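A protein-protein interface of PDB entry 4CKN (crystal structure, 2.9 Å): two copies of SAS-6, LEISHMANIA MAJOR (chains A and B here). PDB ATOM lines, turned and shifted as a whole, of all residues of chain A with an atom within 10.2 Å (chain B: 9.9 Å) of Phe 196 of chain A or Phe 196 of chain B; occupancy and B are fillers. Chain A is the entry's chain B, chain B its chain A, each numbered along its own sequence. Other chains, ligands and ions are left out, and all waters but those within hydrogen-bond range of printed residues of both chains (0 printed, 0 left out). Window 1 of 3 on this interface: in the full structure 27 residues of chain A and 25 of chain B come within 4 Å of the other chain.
Gln 194 of chain A touches none of the printed residues of chain B.
Ser 195 of chain A touches just one residue of chain B: Phe 196 (3.6 Å).
Printed residues of chain B within 4 Å of Phe 196 of chain A: Ser 195 (3.4 Å) and Phe 196 (3.6 Å).
No residue of chain B comes within 4 Å of Ala 198 of chain A.
Of chain B, only Ser 199 (2.4 Å) and Glu 200 (2.8 Å) come within 4 Å of Ser 199 of chain A.
Of the printed residues of chain B, Glu 200 of chain A touches Ser 199.
Ala 204 of chain A touches none of the printed residues of chain B.
Of the printed residues of chain A, Phe 189 of chain B touches Arg 188 (3.6 Å), Phe 189 (3.9 Å) and Tyr 192 (3.5 Å).
Ser 195 of chain B touches one residue of chain A.
Phe 196 of chain B touches just these residues of chain A: Tyr 192, Ser 195 and Phe 196.
Arg 197 of chain B touches just one residue of chain A: Tyr 192 (3.6 Å).
No residue of chain A comes within 4 Å of Ala 198 of chain B.
Ser 199 of chain B touches just these residues of chain A: Ser 199, Glu 200 and Arg 203.
Of the printed residues of chain A, Ser 202 of chain B touches Arg 203.
The nearest printed residue of chain B that does not touch Phe 196 of chain A is Tyr 192 of chain B (4.01 Å).
The nearest residue of chain A that does not touch Phe 196 of chain B is Ser 199 of chain A (4.2 Å).
Phe 189 of chain A touches Tyr 192 of chain B, and with the chains exchanged Tyr 192 of chain A touches Phe 189 of chain B.
Tyr 192 of chain B touches its own counterpart, Tyr 192 of chain A.
Ser 195 of chain A touches Phe 196 of chain B, and with the chains exchanged Phe 196 of chain A touches Ser 195 of chain B.
Phe 196 of chain A touches its own counterpart, Phe 196 of chain B.
Of the 17 printed residues of chain A, 11 touch a printed residue of chain B.
Hydrophobic or aromatic side chains of chain A that line the printed part of chain B: Phe 189, Tyr 192 and Phe 196.
Of the 17 printed residues of chain B, 11 touch a printed residue of chain A.
Hydrophobic or aromatic side chains of chain B within 4 Å of the printed part of chain A: Phe 189, Tyr 192 and Phe 196.
Among the printed residues, no Asp or Glu carboxylate lies within 4 Å of a Lys or Arg side-chain nitrogen of the other chain.
The side-chain hydroxyl (OH) of Tyr 192 of chain B lies within hydrogen-bond range of the side-chain carboxylate (OE2) of Glu 193 of chain A (3.1 Å).
The side-chain carboxylate (OE2) of Glu 193 of chain B lies within hydrogen-bond range of the side-chain hydroxyl (OH) of Tyr 192 of chain A (3.4 Å).
The side-chain hydroxyl (OG) of Ser 199 of chain B sits at hydrogen-bond distance from the side-chain hydroxyl (OG) of Ser 199 of chain A, at 2.4 Å.
The side-chain hydroxyl of Ser 199 of chain B is in hydrogen-bond range of the side-chain carboxylate of Glu 200 of chain A (2.7 Å).
OE1 of Glu 200 of chain B is in hydrogen-bond range of OG of Ser 199 of chain A, at 2.8 Å.
The guanidinium group (NH2) of Arg 203 of chain B is in hydrogen-bond range of the side-chain hydroxyl (OG) of Ser 202 of chain A (2.9 Å).
The side-chain hydroxyl of Ser 195 of chain B sits at hydrogen-bond distance from the backbone carbonyl oxygen of His 191 of chain B (2.9 Å).
OE2 of Glu 193 of chain B is in salt-bridge range of NH2 of Arg 197 of chain B (3.9 Å).
The side-chain carboxylate (OE1) of Glu 200 of chain B is in salt-bridge range of the guanidinium group (NH1) of Arg 203 of chain B.
The side-chain carboxylate (OE2) of Glu 193 of chain A is in salt-bridge range of the guanidinium group (NH2) of Arg 197 of chain A (3.9 Å).
OG of Ser 202 of chain A sits at hydrogen-bond distance from O of Ser 199 of chain A, 3.3 Å away.
Phe 189 of chain B touches Arg 188 of chain A (CD1 to CB, 3.6 Å).
Phe 189 of chain A touches Phe 189 of chain B (CB to CB, 3.9 Å).
Tyr 192 of chain A touches Phe 189 of chain B.
Tyr 192 of chain A touches Phe 196 of chain B (CD1 to CD2, 3.9 Å).
NH2 of Arg 197 of chain B touches OH of Tyr 192 of chain A, at 3.6 Å.
Phe 196 of chain B touches Ser 195 of chain A.
O of Ser 195 of chain B touches CD1 of Phe 196 of chain A, at 3.4 Å.
Phe 196 of chain A touches Phe 196 of chain B.
O of Ser 199 of chain B touches CD of Arg 203 of chain A (3.8 Å).
NE of Arg 203 of chain A touches OG of Ser 202 of chain B (3.7 Å).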
ATOM      1  N   ARG A 188     -29.035   0.899  19.085  1.00  0.00           N
ATOM      2  CA  ARG A 188     -27.744   0.607  19.704  1.00  0.00           C
ATOM      3  C   ARG A 188     -27.051  -0.512  18.954  1.00  0.00           C
ATOM      4  O   ARG A 188     -25.875  -0.408  18.609  1.00  0.00           O
ATOM      5  CB  ARG A 188     -27.903   0.188  21.171  1.00  0.00           C
ATOM      6  CG  ARG A 188     -28.303   1.252  22.171  1.00  0.00           C
ATOM      7  CD  ARG A 188     -27.168   2.221  22.427  1.00  0.00           C
ATOM      8  NE  ARG A 188     -26.986   3.154  21.331  1.00  0.00           N
ATOM      9  CZ  ARG A 188     -25.857   3.809  21.052  1.00  0.00           C
ATOM     10  NH1 ARG A 188     -24.727   3.660  21.765  1.00  0.00           N
ATOM     11  NH2 ARG A 188     -25.854   4.636  20.020  1.00  0.00           N
ATOM     12  N   PHE A 189     -27.793  -1.588  18.730  1.00  0.00           N
ATOM     13  CA  PHE A 189     -27.316  -2.745  17.970  1.00  0.00           C
ATOM     14  C   PHE A 189     -26.758  -2.310  16.625  1.00  0.00           C
ATOM     15  O   PHE A 189     -25.590  -2.554  16.332  1.00  0.00           O
ATOM     16  CB  PHE A 189     -28.453  -3.768  17.838  1.00  0.00           C
ATOM     17  CG  PHE A 189     -28.299  -4.747  16.705  1.00  0.00           C
ATOM     18  CD1 PHE A 189     -27.057  -5.253  16.339  1.00  0.00           C
ATOM     19  CD2 PHE A 189     -29.423  -5.202  16.033  1.00  0.00           C
ATOM     20  CE1 PHE A 189     -26.941  -6.155  15.296  1.00  0.00           C
ATOM     21  CE2 PHE A 189     -29.314  -6.115  14.999  1.00  0.00           C
ATOM     22  CZ  PHE A 189     -28.071  -6.588  14.630  1.00  0.00           C
ATOM     23  N   GLN A 190     -27.569  -1.632  15.828  1.00  0.00           N
ATOM     24  CA  GLN A 190     -27.100  -1.147  14.531  1.00  0.00           C
ATOM     25  C   GLN A 190     -25.843  -0.305  14.678  1.00  0.00           C
ATOM     26  O   GLN A 190     -24.868  -0.516  13.957  1.00  0.00           O
ATOM     27  CB  GLN A 190     -28.169  -0.324  13.821  1.00  0.00           C
ATOM     28  CG  GLN A 190     -29.478  -1.059  13.651  1.00  0.00           C
ATOM     29  CD  GLN A 190     -30.263  -0.567  12.473  1.00  0.00           C
ATOM     30  OE1 GLN A 190     -30.572   0.623  12.382  1.00  0.00           O
ATOM     31  NE2 GLN A 190     -30.616  -1.474  11.574  1.00  0.00           N
ATOM     32  N   HIS A 191     -25.866   0.637  15.617  1.00  0.00           N
ATOM     33  CA  HIS A 191     -24.737   1.525  15.842  1.00  0.00           C
ATOM     34  C   HIS A 191     -23.456   0.749  16.132  1.00  0.00           C
ATOM     35  O   HIS A 191     -22.436   0.983  15.489  1.00  0.00           O
ATOM     36  CB  HIS A 191     -25.028   2.498  16.988  1.00  0.00           C
ATOM     37  CG  HIS A 191     -23.818   3.233  17.487  1.00  0.00           C
ATOM     38  ND1 HIS A 191     -23.038   2.768  18.527  1.00  0.00           N
ATOM     39  CD2 HIS A 191     -23.251   4.395  17.085  1.00  0.00           C
ATOM     40  CE1 HIS A 191     -22.047   3.612  18.750  1.00  0.00           C
ATOM     41  NE2 HIS A 191     -22.153   4.608  17.888  1.00  0.00           N
ATOM     42  N   TYR A 192     -23.497  -0.160  17.094  1.00  0.00           N
ATOM     43  CA  TYR A 192     -22.275  -0.854  17.507  1.00  0.00           C
ATOM     44  C   TYR A 192     -21.784  -1.845  16.465  1.00  0.00           C
ATOM     45  O   TYR A 192     -20.583  -2.026  16.304  1.00  0.00           O
ATOM     46  CB  TYR A 192     -22.432  -1.519  18.878  1.00  0.00           C
ATOM     47  CG  TYR A 192     -22.221  -0.535  19.995  1.00  0.00           C
ATOM     48  CD1 TYR A 192     -20.976   0.049  20.196  1.00  0.00           C
ATOM     49  CD2 TYR A 192     -23.269  -0.147  20.823  1.00  0.00           C
ATOM     50  CE1 TYR A 192     -20.776   0.979  21.200  1.00  0.00           C
ATOM     51  CE2 TYR A 192     -23.074   0.779  21.833  1.00  0.00           C
ATOM     52  CZ  TYR A 192     -21.829   1.336  22.019  1.00  0.00           C
ATOM     53  OH  TYR A 192     -21.639   2.255  23.021  1.00  0.00           O
ATOM     54  N   GLU A 193     -22.701  -2.459  15.731  1.00  0.00           N
ATOM     55  CA  GLU A 193     -22.299  -3.281  14.605  1.00  0.00           C
ATOM     56  C   GLU A 193     -21.559  -2.413  13.597  1.00  0.00           C
ATOM     57  O   GLU A 193     -20.452  -2.737  13.182  1.00  0.00           O
ATOM     58  CB  GLU A 193     -23.506  -3.923  13.937  1.00  0.00           C
ATOM     59  CG  GLU A 193     -23.141  -4.663  12.667  1.00  0.00           C
ATOM     60  CD  GLU A 193     -24.265  -5.519  12.138  1.00  0.00           C
ATOM     61  OE1 GLU A 193     -25.381  -4.967  11.977  1.00  0.00           O
ATOM     62  OE2 GLU A 193     -24.026  -6.733  11.893  1.00  0.00           O
ATOM     63  N   GLN A 194     -22.188  -1.307  13.213  1.00  0.00           N
ATOM     64  CA  GLN A 194     -21.603  -0.367  12.265  1.00  0.00           C
ATOM     65  C   GLN A 194     -20.225   0.069  12.735  1.00  0.00           C
ATOM     66  O   GLN A 194     -19.272   0.084  11.965  1.00  0.00           O
ATOM     67  CB  GLN A 194     -22.509   0.848  12.120  1.00  0.00           C
ATOM     68  CG  GLN A 194     -22.288   1.656  10.860  1.00  0.00           C
ATOM     69  CD  GLN A 194     -23.310   2.773  10.715  1.00  0.00           C
ATOM     70  OE1 GLN A 194     -24.460   2.641  11.147  1.00  0.00           O
ATOM     71  NE2 GLN A 194     -22.896   3.884  10.111  1.00  0.00           N
ATOM     72  N   SER A 195     -20.125   0.395  14.015  1.00  0.00           N
ATOM     73  CA  SER A 195     -18.870   0.822  14.602  1.00  0.00           C
ATOM     74  C   SER A 195     -17.850  -0.301  14.591  1.00  0.00           C
ATOM     75  O   SER A 195     -16.684  -0.081  14.271  1.00  0.00           O
ATOM     76  CB  SER A 195     -19.099   1.301  16.034  1.00  0.00           C
ATOM     77  OG  SER A 195     -20.002   2.389  16.040  1.00  0.00           O
ATOM     78  N   PHE A 196     -18.291  -1.505  14.940  1.00  0.00           N
ATOM     79  CA  PHE A 196     -17.406  -2.668  14.940  1.00  0.00           C
ATOM     80  C   PHE A 196     -16.825  -2.930  13.557  1.00  0.00           C
ATOM     81  O   PHE A 196     -15.645  -3.233  13.434  1.00  0.00           O
ATOM     82  CB  PHE A 196     -18.130  -3.916  15.437  1.00  0.00           C
ATOM     83  CG  PHE A 196     -17.349  -5.179  15.235  1.00  0.00           C
ATOM     84  CD1 PHE A 196     -16.198  -5.419  15.971  1.00  0.00           C
ATOM     85  CD2 PHE A 196     -17.751  -6.118  14.295  1.00  0.00           C
ATOM     86  CE1 PHE A 196     -15.464  -6.578  15.781  1.00  0.00           C
ATOM     87  CE2 PHE A 196     -17.024  -7.280  14.104  1.00  0.00           C
ATOM     88  CZ  PHE A 196     -15.879  -7.511  14.847  1.00  0.00           C
ATOM     89  N   ARG A 197     -17.647  -2.798  12.522  1.00  0.00           N
ATOM     90  CA  ARG A 197     -17.163  -2.935  11.155  1.00  0.00           C
ATOM     91  C   ARG A 197     -16.097  -1.886  10.882  1.00  0.00           C
ATOM     92  O   ARG A 197     -14.977  -2.217  10.483  1.00  0.00           O
ATOM     93  CB  ARG A 197     -18.296  -2.772  10.139  1.00  0.00           C
ATOM     94  CG  ARG A 197     -19.378  -3.840  10.189  1.00  0.00           C
ATOM     95  CD  ARG A 197     -18.855  -5.246   9.948  1.00  0.00           C
ATOM     96  NE  ARG A 197     -19.855  -6.247  10.329  1.00  0.00           N
ATOM     97  CZ  ARG A 197     -19.596  -7.533  10.577  1.00  0.00           C
ATOM     98  NH1 ARG A 197     -18.358  -8.013  10.480  1.00  0.00           N
ATOM     99  NH2 ARG A 197     -20.586  -8.348  10.929  1.00  0.00           N
ATOM    100  N   ALA A 198     -16.443  -0.625  11.121  1.00  0.00           N
ATOM    101  CA  ALA A 198     -15.533   0.488  10.869  1.00  0.00           C
ATOM    102  C   ALA A 198     -14.205   0.311  11.601  1.00  0.00           C
ATOM    103  O   ALA A 198     -13.145   0.570  11.033  1.00  0.00           O
ATOM    104  CB  ALA A 198     -16.179   1.804  11.274  1.00  0.00           C
ATOM    105  N   SER A 199     -14.266  -0.135  12.852  1.00  0.00           N
ATOM    106  CA  SER A 199     -13.060  -0.395  13.631  1.00  0.00           C
ATOM    107  C   SER A 199     -12.149  -1.352  12.890  1.00  0.00           C
ATOM    108  O   SER A 199     -10.985  -1.042  12.660  1.00  0.00           O
ATOM    109  CB  SER A 199     -13.399  -0.972  15.007  1.00  0.00           C
ATOM    110  OG  SER A 199     -12.229  -1.155  15.786  1.00  0.00           O
ATOM    111  N   GLU A 200     -12.696  -2.494  12.487  1.00  0.00           N
ATOM    112  CA  GLU A 200     -11.916  -3.509  11.780  1.00  0.00           C
ATOM    113  C   GLU A 200     -11.345  -2.980  10.463  1.00  0.00           C
ATOM    114  O   GLU A 200     -10.174  -3.202  10.149  1.00  0.00           O
ATOM    115  CB  GLU A 200     -12.768  -4.758  11.503  1.00  0.00           C
ATOM    116  CG  GLU A 200     -13.282  -5.483  12.738  1.00  0.00           C
ATOM    117  CD  GLU A 200     -12.182  -6.124  13.564  1.00  0.00           C
ATOM    118  OE1 GLU A 200     -11.346  -5.392  14.138  1.00  0.00           O
ATOM    119  OE2 GLU A 200     -12.155  -7.370  13.640  1.00  0.00           O
ATOM    120  N   ALA A 201     -12.185  -2.289   9.697  1.00  0.00           N
ATOM    121  CA  ALA A 201     -11.776  -1.715   8.418  1.00  0.00           C
ATOM    122  C   ALA A 201     -10.539  -0.840   8.590  1.00  0.00           C
ATOM    123  O   ALA A 201      -9.522  -1.049   7.924  1.00  0.00           O
ATOM    124  CB  ALA A 201     -12.915  -0.908   7.822  1.00  0.00           C
ATOM    125  N   SER A 202     -10.615   0.098   9.528  1.00  0.00           N
ATOM    126  CA  SER A 202      -9.516   1.025   9.773  1.00  0.00           C
ATOM    127  C   SER A 202      -8.350   0.354  10.505  1.00  0.00           C
ATOM    128  O   SER A 202      -7.233   0.865  10.486  1.00  0.00           O
ATOM    129  CB  SER A 202      -9.991   2.232  10.583  1.00  0.00           C
ATOM    130  OG  SER A 202      -9.890   1.976  11.972  1.00  0.00           O
ATOM    131  N   ARG A 203      -8.605  -0.768  11.172  1.00  0.00           N
ATOM    132  CA  ARG A 203      -7.531  -1.532  11.786  1.00  0.00           C
ATOM    133  C   ARG A 203      -6.682  -2.175  10.700  1.00  0.00           C
ATOM    134  O   ARG A 203      -5.456  -2.038  10.698  1.00  0.00           O
ATOM    135  CB  ARG A 203      -8.069  -2.613  12.710  1.00  0.00           C
ATOM    136  CG  ARG A 203      -7.022  -2.996  13.735  1.00  0.00           C
ATOM    137  CD  ARG A 203      -7.578  -3.745  14.945  1.00  0.00           C
ATOM    138  NE  ARG A 203      -8.332  -4.949  14.601  1.00  0.00           N
ATOM    139  CZ  ARG A 203      -7.805  -6.141  14.323  1.00  0.00           C
ATOM    140  NH1 ARG A 203      -6.487  -6.326  14.319  1.00  0.00           N
ATOM    141  NH2 ARG A 203      -8.607  -7.163  14.035  1.00  0.00           N
ATOM    142  N   ALA A 204      -7.347  -2.865   9.775  1.00  0.00           N
ATOM    143  CA  ALA A 204      -6.682  -3.502   8.638  1.00  0.00           C
ATOM    144  C   ALA A 204      -5.860  -2.497   7.830  1.00  0.00           C
ATOM    145  O   ALA A 204      -4.733  -2.790   7.416  1.00  0.00           O
ATOM    146  CB  ALA A 204      -7.710  -4.170   7.746  1.00  0.00           C
ATOM    147  N   ARG B 188     -27.710  -9.135  20.473  1.00  0.00           N
ATOM    148  CA  ARG B 188     -26.943  -8.618  19.338  1.00  0.00           C
ATOM    149  C   ARG B 188     -26.195  -7.369  19.744  1.00  0.00           C
ATOM    150  O   ARG B 188     -24.994  -7.243  19.507  1.00  0.00           O
ATOM    151  CB  ARG B 188     -27.846  -8.272  18.151  1.00  0.00           C
ATOM    152  CG  ARG B 188     -28.466  -9.416  17.382  1.00  0.00           C
ATOM    153  CD  ARG B 188     -27.425 -10.164  16.552  1.00  0.00           C
ATOM    154  NE  ARG B 188     -26.575 -11.019  17.373  1.00  0.00           N
ATOM    155  CZ  ARG B 188     -25.344 -11.440  17.064  1.00  0.00           C
ATOM    156  NH1 ARG B 188     -24.733 -11.103  15.923  1.00  0.00           N
ATOM    157  NH2 ARG B 188     -24.706 -12.218  17.929  1.00  0.00           N
ATOM    158  N   PHE B 189     -26.930  -6.450  20.352  1.00  0.00           N
ATOM    159  CA  PHE B 189     -26.376  -5.212  20.871  1.00  0.00           C
ATOM    160  C   PHE B 189     -25.188  -5.499  21.781  1.00  0.00           C
ATOM    161  O   PHE B 189     -24.093  -5.020  21.527  1.00  0.00           O
ATOM    162  CB  PHE B 189     -27.488  -4.426  21.575  1.00  0.00           C
ATOM    163  CG  PHE B 189     -27.012  -3.369  22.526  1.00  0.00           C
ATOM    164  CD1 PHE B 189     -25.869  -2.619  22.280  1.00  0.00           C
ATOM    165  CD2 PHE B 189     -27.760  -3.085  23.657  1.00  0.00           C
ATOM    166  CE1 PHE B 189     -25.463  -1.639  23.168  1.00  0.00           C
ATOM    167  CE2 PHE B 189     -27.361  -2.102  24.538  1.00  0.00           C
ATOM    168  CZ  PHE B 189     -26.211  -1.380  24.294  1.00  0.00           C
ATOM    169  N   GLN B 190     -25.391  -6.302  22.818  1.00  0.00           N
ATOM    170  CA  GLN B 190     -24.298  -6.647  23.726  1.00  0.00           C
ATOM    171  C   GLN B 190     -23.118  -7.236  22.967  1.00  0.00           C
ATOM    172  O   GLN B 190     -21.983  -6.826  23.168  1.00  0.00           O
ATOM    173  CB  GLN B 190     -24.744  -7.624  24.817  1.00  0.00           C
ATOM    174  CG  GLN B 190     -25.933  -7.135  25.633  1.00  0.00           C
ATOM    175  CD  GLN B 190     -25.868  -7.528  27.103  1.00  0.00           C
ATOM    176  OE1 GLN B 190     -25.231  -6.835  27.894  1.00  0.00           O
ATOM    177  NE2 GLN B 190     -26.534  -8.621  27.482  1.00  0.00           N
ATOM    178  N   HIS B 191     -23.396  -8.186  22.083  1.00  0.00           N
ATOM    179  CA  HIS B 191     -22.352  -8.850  21.304  1.00  0.00           C
ATOM    180  C   HIS B 191     -21.514  -7.860  20.504  1.00  0.00           C
ATOM    181  O   HIS B 191     -20.296  -7.869  20.591  1.00  0.00           O
ATOM    182  CB  HIS B 191     -22.963  -9.890  20.362  1.00  0.00           C
ATOM    183  CG  HIS B 191     -22.012 -10.395  19.321  1.00  0.00           C
ATOM    184  ND1 HIS B 191     -21.911  -9.825  18.070  1.00  0.00           N
ATOM    185  CD2 HIS B 191     -21.118 -11.411  19.346  1.00  0.00           C
ATOM    186  CE1 HIS B 191     -20.998 -10.471  17.366  1.00  0.00           C
ATOM    187  NE2 HIS B 191     -20.501 -11.438  18.117  1.00  0.00           N
ATOM    188  N   TYR B 192     -22.167  -7.001  19.731  1.00  0.00           N
ATOM    189  CA  TYR B 192     -21.432  -6.096  18.863  1.00  0.00           C
ATOM    190  C   TYR B 192     -20.715  -4.996  19.637  1.00  0.00           C
ATOM    191  O   TYR B 192     -19.636  -4.563  19.240  1.00  0.00           O
ATOM    192  CB  TYR B 192     -22.327  -5.521  17.769  1.00  0.00           C
ATOM    193  CG  TYR B 192     -22.482  -6.485  16.622  1.00  0.00           C
ATOM    194  CD1 TYR B 192     -21.387  -6.830  15.834  1.00  0.00           C
ATOM    195  CD2 TYR B 192     -23.704  -7.078  16.336  1.00  0.00           C
ATOM    196  CE1 TYR B 192     -21.515  -7.726  14.788  1.00  0.00           C
ATOM    197  CE2 TYR B 192     -23.840  -7.974  15.290  1.00  0.00           C
ATOM    198  CZ  TYR B 192     -22.743  -8.292  14.523  1.00  0.00           C
ATOM    199  OH  TYR B 192     -22.881  -9.181  13.491  1.00  0.00           O
ATOM    200  N   GLU B 193     -21.295  -4.556  20.747  1.00  0.00           N
ATOM    201  CA  GLU B 193     -20.600  -3.637  21.623  1.00  0.00           C
ATOM    202  C   GLU B 193     -19.332  -4.310  22.128  1.00  0.00           C
ATOM    203  O   GLU B 193     -18.250  -3.757  22.027  1.00  0.00           O
ATOM    204  CB  GLU B 193     -21.474  -3.226  22.801  1.00  0.00           C
ATOM    205  CG  GLU B 193     -20.733  -2.394  23.825  1.00  0.00           C
ATOM    206  CD  GLU B 193     -21.646  -1.750  24.842  1.00  0.00           C
ATOM    207  OE1 GLU B 193     -22.460  -2.482  25.435  1.00  0.00           O
ATOM    208  OE2 GLU B 193     -21.562  -0.519  25.048  1.00  0.00           O
ATOM    209  N   GLN B 194     -19.486  -5.512  22.665  1.00  0.00           N
ATOM    210  CA  GLN B 194     -18.365  -6.297  23.176  1.00  0.00           C
ATOM    211  C   GLN B 194     -17.295  -6.447  22.105  1.00  0.00           C
ATOM    212  O   GLN B 194     -16.120  -6.245  22.366  1.00  0.00           O
ATOM    213  CB  GLN B 194     -18.854  -7.673  23.616  1.00  0.00           C
ATOM    214  CG  GLN B 194     -17.932  -8.406  24.568  1.00  0.00           C
ATOM    215  CD  GLN B 194     -18.542  -9.711  25.061  1.00  0.00           C
ATOM    216  OE1 GLN B 194     -19.759  -9.813  25.235  1.00  0.00           O
ATOM    217  NE2 GLN B 194     -17.700 -10.709  25.304  1.00  0.00           N
ATOM    218  N   SER B 195     -17.723  -6.776  20.894  1.00  0.00           N
ATOM    219  CA  SER B 195     -16.817  -6.944  19.772  1.00  0.00           C
ATOM    220  C   SER B 195     -16.148  -5.628  19.407  1.00  0.00           C
ATOM    221  O   SER B 195     -14.939  -5.578  19.162  1.00  0.00           O
ATOM    222  CB  SER B 195     -17.576  -7.502  18.569  1.00  0.00           C
ATOM    223  OG  SER B 195     -18.161  -8.760  18.885  1.00  0.00           O
ATOM    224  N   PHE B 196     -16.930  -4.553  19.385  1.00  0.00           N
ATOM    225  CA  PHE B 196     -16.386  -3.226  19.095  1.00  0.00           C
ATOM    226  C   PHE B 196     -15.313  -2.827  20.104  1.00  0.00           C
ATOM    227  O   PHE B 196     -14.297  -2.258  19.725  1.00  0.00           O
ATOM    228  CB  PHE B 196     -17.492  -2.172  19.069  1.00  0.00           C
ATOM    229  CG  PHE B 196     -16.980  -0.761  19.004  1.00  0.00           C
ATOM    230  CD1 PHE B 196     -16.356  -0.287  17.863  1.00  0.00           C
ATOM    231  CD2 PHE B 196     -17.114   0.091  20.092  1.00  0.00           C
ATOM    232  CE1 PHE B 196     -15.876   1.011  17.806  1.00  0.00           C
ATOM    233  CE2 PHE B 196     -16.641   1.390  20.044  1.00  0.00           C
ATOM    234  CZ  PHE B 196     -16.019   1.850  18.896  1.00  0.00           C
ATOM    235  N   ARG B 197     -15.542  -3.116  21.382  1.00  0.00           N
ATOM    236  CA  ARG B 197     -14.543  -2.846  22.403  1.00  0.00           C
ATOM    237  C   ARG B 197     -13.284  -3.627  22.094  1.00  0.00           C
ATOM    238  O   ARG B 197     -12.204  -3.050  21.994  1.00  0.00           O
ATOM    239  CB  ARG B 197     -15.040  -3.221  23.802  1.00  0.00           C
ATOM    240  CG  ARG B 197     -16.214  -2.398  24.321  1.00  0.00           C
ATOM    241  CD  ARG B 197     -15.920  -0.908  24.413  1.00  0.00           C
ATOM    242  NE  ARG B 197     -17.149  -0.143  24.614  1.00  0.00           N
ATOM    243  CZ  ARG B 197     -17.283   1.164  24.381  1.00  0.00           C
ATOM    244  NH1 ARG B 197     -16.261   1.892  23.931  1.00  0.00           N
ATOM    245  NH2 ARG B 197     -18.456   1.751  24.594  1.00  0.00           N
ATOM    246  N   ALA B 198     -13.438  -4.938  21.923  1.00  0.00           N
ATOM    247  CA  ALA B 198     -12.307  -5.825  21.663  1.00  0.00           C
ATOM    248  C   ALA B 198     -11.503  -5.362  20.452  1.00  0.00           C
ATOM    249  O   ALA B 198     -10.273  -5.360  20.486  1.00  0.00           O
ATOM    250  CB  ALA B 198     -12.781  -7.256  21.467  1.00  0.00           C
ATOM    251  N   SER B 199     -12.197  -4.960  19.392  1.00  0.00           N
ATOM    252  CA  SER B 199     -11.529  -4.433  18.206  1.00  0.00           C
ATOM    253  C   SER B 199     -10.611  -3.269  18.577  1.00  0.00           C
ATOM    254  O   SER B 199      -9.431  -3.280  18.257  1.00  0.00           O
ATOM    255  CB  SER B 199     -12.548  -3.982  17.162  1.00  0.00           C
ATOM    256  OG  SER B 199     -11.898  -3.558  15.973  1.00  0.00           O
ATOM    257  N   GLU B 200     -11.155  -2.280  19.281  1.00  0.00           N
ATOM    258  CA  GLU B 200     -10.384  -1.098  19.687  1.00  0.00           C
ATOM    259  C   GLU B 200      -9.221  -1.467  20.608  1.00  0.00           C
ATOM    260  O   GLU B 200      -8.105  -0.983  20.433  1.00  0.00           O
ATOM    261  CB  GLU B 200     -11.284  -0.075  20.388  1.00  0.00           C
ATOM    262  CG  GLU B 200     -12.420   0.493  19.542  1.00  0.00           C
ATOM    263  CD  GLU B 200     -11.947   1.367  18.394  1.00  0.00           C
ATOM    264  OE1 GLU B 200     -11.301   0.844  17.464  1.00  0.00           O
ATOM    265  OE2 GLU B 200     -12.225   2.580  18.420  1.00  0.00           O
ATOM    266  N   ALA B 201      -9.486  -2.334  21.577  1.00  0.00           N
ATOM    267  CA  ALA B 201      -8.457  -2.799  22.505  1.00  0.00           C
ATOM    268  C   ALA B 201      -7.255  -3.353  21.744  1.00  0.00           C
ATOM    269  O   ALA B 201      -6.123  -2.921  21.957  1.00  0.00           O
ATOM    270  CB  ALA B 201      -9.022  -3.858  23.436  1.00  0.00           C
ATOM    271  N   SER B 202      -7.517  -4.281  20.828  1.00  0.00           N
ATOM    272  CA  SER B 202      -6.454  -4.915  20.052  1.00  0.00           C
ATOM    273  C   SER B 202      -5.876  -3.980  18.983  1.00  0.00           C
ATOM    274  O   SER B 202      -4.771  -4.211  18.498  1.00  0.00           O
ATOM    275  CB  SER B 202      -6.955  -6.197  19.384  1.00  0.00           C
ATOM    276  OG  SER B 202      -7.504  -5.917  18.108  1.00  0.00           O
ATOM    277  N   ARG B 203      -6.626  -2.949  18.597  1.00  0.00           N
ATOM    278  CA  ARG B 203      -6.107  -1.931  17.679  1.00  0.00           C
ATOM    279  C   ARG B 203      -5.046  -1.122  18.414  1.00  0.00           C
ATOM    280  O   ARG B 203      -3.933  -0.964  17.925  1.00  0.00           O
ATOM    281  CB  ARG B 203      -7.229  -1.006  17.189  1.00  0.00           C
ATOM    282  CG  ARG B 203      -6.936  -0.115  15.984  1.00  0.00           C
ATOM    283  CD  ARG B 203      -7.619   1.217  16.162  1.00  0.00           C
ATOM    284  NE  ARG B 203      -7.726   1.995  14.939  1.00  0.00           N
ATOM    285  CZ  ARG B 203      -8.427   3.120  14.852  1.00  0.00           C
ATOM    286  NH1 ARG B 203      -9.080   3.590  15.913  1.00  0.00           N
ATOM    287  NH2 ARG B 203      -8.479   3.778  13.705  1.00  0.00           N
ATOM    288  N   ALA B 204      -5.397  -0.631  19.602  1.00  0.00           N
ATOM    289  CA  ALA B 204      -4.479   0.136  20.449  1.00  0.00           C
ATOM    290  C   ALA B 204      -3.203  -0.646  20.744  1.00  0.00           C
ATOM    291  O   ALA B 204      -2.106  -0.091  20.708  1.00  0.00           O
ATOM    292  CB  ALA B 204      -5.162   0.534  21.747  1.00  0.00           C
